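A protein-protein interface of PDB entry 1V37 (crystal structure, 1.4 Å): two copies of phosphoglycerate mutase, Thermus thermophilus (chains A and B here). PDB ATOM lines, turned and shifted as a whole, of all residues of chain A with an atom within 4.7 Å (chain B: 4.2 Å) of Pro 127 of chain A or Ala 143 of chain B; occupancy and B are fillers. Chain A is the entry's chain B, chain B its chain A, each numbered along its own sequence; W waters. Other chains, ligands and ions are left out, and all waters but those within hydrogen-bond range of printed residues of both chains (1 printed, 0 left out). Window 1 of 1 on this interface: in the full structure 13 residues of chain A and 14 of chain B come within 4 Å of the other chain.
N of Ala 126 of chain A lies close to SD of Met 1 of chain A (3.5 Å).
Among the printed residues, pairs that only touch across the chains: Met 1 of chain A with Pro 161 of chain B, Leu 45 of chain A with Arg 142 of chain B, Leu 45 of chain A with Ala 143 of chain B, Leu 45 of chain A with Gly 145 of chain B, Ala 126 of chain A with Phe 118 of chain B, Pro 127 of chain A with Ala 143 of chain B and Pro 127 of chain A with Pro 161 of chain B.
Pro 127 of chain A touches two residues of chain B. Ala 143 of chain B touches just these residues of chain A: Leu 45 and Pro 127. Of the printed residues of chain A, Arg 142 of chain B touches Leu 45 (3.5 Å). Printed residues of chain A within 4 Å of Gly 145 of chain B: Leu 45 (3.9 Å). Printed residues of chain B within 4 Å of Ala 126 of chain A: Phe 118 (3.6 Å). Of the printed residues of chain A, Pro 161 of chain B touches Met 1 and Pro 127. Val 140 of chain B touches none of the printed residues of chain A. Ala 128 of chain A touches none of the printed residues of chain B. The nearest printed residue of chain B that does not touch Pro 127 of chain A is Leu 144 of chain B (4.4 Å). The nearest residue of chain A that does not touch Ala 143 of chain B is Pro 46 of chain A (4.1 Å). The nearest printed residue of chain A that does not touch Pro 161 of chain B is Ala 126 of chain A (4.8 Å).
Of the 9 printed residues of chain B, 5 touch a printed residue of chain A. Printed residues of chain B that touch a printed residue of chain A: Phe 118, Arg 142, Ala 143, Gly 145 and Pro 161. Hydrophobic or aromatic side chains of chain B within 4 Å of the printed part of chain A: Phe 118 and Pro 161. Of the 8 printed residues of chain A, 4 touch a printed residue of chain B. Hydrophobic or aromatic side chains of chain A within 4 Å of the printed part of chain B: Met 1, Leu 45, Ala 126 and Pro 127.
No position is printed for both chains.
Water W1 lies within hydrogen-bond range of O of Pro 161 of chain B (2.8 Å) and N of Glu 2 of chain A (2.9 Å).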
ATOM      1  N   MET A   1      14.455  -5.845   4.007  1.00  0.00           N
ATOM      2  CA  MET A   1      13.565  -7.033   4.095  1.00  0.00           C
ATOM      3  C   MET A   1      12.596  -6.847   5.256  1.00  0.00           C
ATOM      4  O   MET A   1      13.005  -6.556   6.382  1.00  0.00           O
ATOM      5  CB  MET A   1      14.402  -8.288   4.291  1.00  0.00           C
ATOM      6  CG  MET A   1      13.608  -9.557   4.127  1.00  0.00           C
ATOM      7  SD  MET A   1      14.673 -10.984   4.014  1.00  0.00           S
ATOM      8  CE  MET A   1      15.090 -11.202   5.733  1.00  0.00           C
ATOM      9  N   GLU A   2      11.313  -7.028   4.971  1.00  0.00           N
ATOM     10  CA  GLU A   2      10.266  -6.822   5.960  1.00  0.00           C
ATOM     11  C   GLU A   2      10.216  -7.839   7.090  1.00  0.00           C
ATOM     12  O   GLU A   2      10.051  -9.037   6.858  1.00  0.00           O
ATOM     13  CB  GLU A   2       8.908  -6.763   5.257  1.00  0.00           C
ATOM     14  CG  GLU A   2       7.774  -6.281   6.145  1.00  0.00           C
ATOM     15  CD  GLU A   2       6.500  -6.029   5.371  1.00  0.00           C
ATOM     16  OE1 GLU A   2       6.598  -5.552   4.218  1.00  0.00           O
ATOM     17  OE2 GLU A   2       5.403  -6.291   5.911  1.00  0.00           O
ATOM     18  N   LEU A   3      10.350  -7.347   8.317  1.00  0.00           N
ATOM     19  CA  LEU A   3      10.293  -8.193   9.503  1.00  0.00           C
ATOM     20  C   LEU A   3       9.329  -7.579  10.502  1.00  0.00           C
ATOM     21  O   LEU A   3       9.394  -6.377  10.783  1.00  0.00           O
ATOM     22  CB  LEU A   3      11.667  -8.311  10.174  1.00  0.00           C
ATOM     23  CG  LEU A   3      12.857  -8.840   9.371  1.00  0.00           C
ATOM     24  CD1 LEU A   3      14.071  -8.875  10.288  1.00  0.00           C
ATOM     25  CD2 LEU A   3      12.571 -10.228   8.810  1.00  0.00           C
ATOM     26  N   LEU A  45       3.166 -14.023   6.820  1.00  0.00           N
ATOM     27  CA  LEU A  45       4.525 -14.291   6.366  1.00  0.00           C
ATOM     28  C   LEU A  45       5.060 -15.470   7.175  1.00  0.00           C
ATOM     29  O   LEU A  45       4.454 -15.874   8.168  1.00  0.00           O
ATOM     30  CB  LEU A  45       5.425 -13.078   6.639  1.00  0.00           C
ATOM     31  CG  LEU A  45       4.869 -11.694   6.303  1.00  0.00           C
ATOM     32  CD1 LEU A  45       5.908 -10.627   6.630  1.00  0.00           C
ATOM     33  CD2 LEU A  45       4.495 -11.635   4.823  1.00  0.00           C
ATOM     34  N   PRO A  46       6.193 -16.050   6.749  1.00  0.00           N
ATOM     35  CA  PRO A  46       6.772 -17.175   7.490  1.00  0.00           C
ATOM     36  C   PRO A  46       6.948 -16.709   8.939  1.00  0.00           C
ATOM     37  O   PRO A  46       7.397 -15.583   9.181  1.00  0.00           O
ATOM     38  CB  PRO A  46       8.108 -17.395   6.787  1.00  0.00           C
ATOM     39  CG  PRO A  46       7.795 -17.020   5.359  1.00  0.00           C
ATOM     40  CD  PRO A  46       6.957 -15.770   5.519  1.00  0.00           C
ATOM     41  N   ALA A 126      14.122 -14.474   4.230  1.00  0.00           N
ATOM     42  CA  ALA A 126      12.882 -14.001   3.643  1.00  0.00           C
ATOM     43  C   ALA A 126      12.124 -13.211   4.699  1.00  0.00           C
ATOM     44  O   ALA A 126      12.432 -13.302   5.890  1.00  0.00           O
ATOM     45  CB  ALA A 126      12.034 -15.187   3.166  1.00  0.00           C
ATOM     46  N   PRO A 127      11.144 -12.398   4.275  1.00  0.00           N
ATOM     47  CA  PRO A 127      10.355 -11.613   5.228  1.00  0.00           C
ATOM     48  C   PRO A 127       9.752 -12.571   6.245  1.00  0.00           C
ATOM     49  O   PRO A 127       9.509 -13.745   5.937  1.00  0.00           O
ATOM     50  CB  PRO A 127       9.301 -10.963   4.345  1.00  0.00           C
ATOM     51  CG  PRO A 127      10.056 -10.723   3.075  1.00  0.00           C
ATOM     52  CD  PRO A 127      10.804 -12.031   2.888  1.00  0.00           C
ATOM     53  N   ALA A 128       9.497 -12.080   7.451  1.00  0.00           N
ATOM     54  CA  ALA A 128       8.974 -12.944   8.491  1.00  0.00           C
ATOM     55  C   ALA A 128       8.284 -12.193   9.610  1.00  0.00           C
ATOM     56  O   ALA A 128       8.446 -10.979   9.756  1.00  0.00           O
ATOM     57  CB  ALA A 128      10.120 -13.773   9.074  1.00  0.00           C
ATOM     58  N   PHE B 118      14.107 -20.598   0.081  1.00  0.00           N
ATOM     59  CA  PHE B 118      14.715 -19.312   0.384  1.00  0.00           C
ATOM     60  C   PHE B 118      16.236 -19.364   0.448  1.00  0.00           C
ATOM     61  O   PHE B 118      16.903 -18.381   0.119  1.00  0.00           O
ATOM     62  CB  PHE B 118      14.114 -18.727   1.666  1.00  0.00           C
ATOM     63  CG  PHE B 118      12.619 -18.529   1.599  1.00  0.00           C
ATOM     64  CD1 PHE B 118      11.999 -18.161   0.404  1.00  0.00           C
ATOM     65  CD2 PHE B 118      11.832 -18.706   2.730  1.00  0.00           C
ATOM     66  CE1 PHE B 118      10.611 -17.975   0.342  1.00  0.00           C
ATOM     67  CE2 PHE B 118      10.447 -18.522   2.675  1.00  0.00           C
ATOM     68  CZ  PHE B 118       9.841 -18.158   1.480  1.00  0.00           C
ATOM     69  N   ALA B 139       5.147 -19.696  -2.192  1.00  0.00           N
ATOM     70  CA  ALA B 139       5.953 -19.389  -1.016  1.00  0.00           C
ATOM     71  C   ALA B 139       6.598 -18.011  -1.142  1.00  0.00           C
ATOM     72  O   ALA B 139       6.639 -17.235  -0.184  1.00  0.00           O
ATOM     73  CB  ALA B 139       7.032 -20.459  -0.830  1.00  0.00           C
ATOM     74  N   VAL B 140       7.106 -17.719  -2.335  1.00  0.00           N
ATOM     75  CA  VAL B 140       7.758 -16.450  -2.611  1.00  0.00           C
ATOM     76  C   VAL B 140       6.770 -15.289  -2.544  1.00  0.00           C
ATOM     77  O   VAL B 140       7.019 -14.297  -1.854  1.00  0.00           O
ATOM     78  CB  VAL B 140       8.429 -16.495  -4.005  1.00  0.00           C
ATOM     79  CG1 VAL B 140       8.857 -15.102  -4.441  1.00  0.00           C
ATOM     80  CG2 VAL B 140       9.633 -17.415  -3.957  1.00  0.00           C
ATOM     81  N   LEU B 141       5.650 -15.412  -3.251  1.00  0.00           N
ATOM     82  CA  LEU B 141       4.651 -14.347  -3.257  1.00  0.00           C
ATOM     83  C   LEU B 141       4.083 -14.107  -1.866  1.00  0.00           C
ATOM     84  O   LEU B 141       3.920 -12.953  -1.452  1.00  0.00           O
ATOM     85  CB  LEU B 141       3.532 -14.676  -4.249  1.00  0.00           C
ATOM     86  CG  LEU B 141       3.937 -14.620  -5.727  1.00  0.00           C
ATOM     87  CD1 LEU B 141       2.760 -15.025  -6.598  1.00  0.00           C
ATOM     88  CD2 LEU B 141       4.418 -13.219  -6.085  1.00  0.00           C
ATOM     89  N   ARG B 142       3.791 -15.180  -1.135  1.00  0.00           N
ATOM     90  CA  ARG B 142       3.247 -15.031   0.215  1.00  0.00           C
ATOM     91  C   ARG B 142       4.249 -14.360   1.149  1.00  0.00           C
ATOM     92  O   ARG B 142       3.870 -13.559   2.000  1.00  0.00           O
ATOM     93  CB  ARG B 142       2.845 -16.383   0.804  1.00  0.00           C
ATOM     94  CG  ARG B 142       1.599 -16.994   0.206  1.00  0.00           C
ATOM     95  CD  ARG B 142       1.211 -18.249   0.968  1.00  0.00           C
ATOM     96  NE  ARG B 142       0.836 -17.978   2.358  1.00  0.00           N
ATOM     97  CZ  ARG B 142      -0.399 -17.690   2.764  1.00  0.00           C
ATOM     98  NH1 ARG B 142      -1.396 -17.628   1.891  1.00  0.00           N
ATOM     99  NH2 ARG B 142      -0.644 -17.482   4.050  1.00  0.00           N
ATOM    100  N   ALA B 143       5.529 -14.675   0.990  1.00  0.00           N
ATOM    101  CA  ALA B 143       6.556 -14.070   1.831  1.00  0.00           C
ATOM    102  C   ALA B 143       6.638 -12.576   1.537  1.00  0.00           C
ATOM    103  O   ALA B 143       7.047 -11.791   2.390  1.00  0.00           O
ATOM    104  CB  ALA B 143       7.906 -14.737   1.584  1.00  0.00           C
ATOM    105  N   LEU B 144       6.247 -12.190   0.324  1.00  0.00           N
ATOM    106  CA  LEU B 144       6.254 -10.786  -0.078  1.00  0.00           C
ATOM    107  C   LEU B 144       4.900 -10.143   0.220  1.00  0.00           C
ATOM    108  O   LEU B 144       4.614  -9.033  -0.231  1.00  0.00           O
ATOM    109  CB  LEU B 144       6.601 -10.661  -1.567  1.00  0.00           C
ATOM    110  CG  LEU B 144       8.029 -11.115  -1.910  1.00  0.00           C
ATOM    111  CD1 LEU B 144       8.241 -11.043  -3.412  1.00  0.00           C
ATOM    112  CD2 LEU B 144       9.042 -10.242  -1.182  1.00  0.00           C
ATOM    113  N   GLY B 145       4.076 -10.865   0.977  1.00  0.00           N
ATOM    114  CA  GLY B 145       2.772 -10.363   1.387  1.00  0.00           C
ATOM    115  C   GLY B 145       1.648 -10.335   0.371  1.00  0.00           C
ATOM    116  O   GLY B 145       0.695  -9.572   0.535  1.00  0.00           O
ATOM    117  N   PRO B 161      14.572  -9.710  -1.750  1.00  0.00           N
ATOM    118  CA  PRO B 161      13.375 -10.129  -1.004  1.00  0.00           C
ATOM    119  C   PRO B 161      12.497  -8.939  -0.600  1.00  0.00           C
ATOM    120  O   PRO B 161      12.069  -8.848   0.552  1.00  0.00           O
ATOM    121  CB  PRO B 161      13.988 -10.794   0.215  1.00  0.00           C
ATOM    122  CG  PRO B 161      15.102  -9.811   0.545  1.00  0.00           C
ATOM    123  CD  PRO B 161      15.678  -9.413  -0.819  1.00  0.00           C
HETATM  124  O   HOH W   1      10.500  -7.298   2.228  1.00  0.00           O
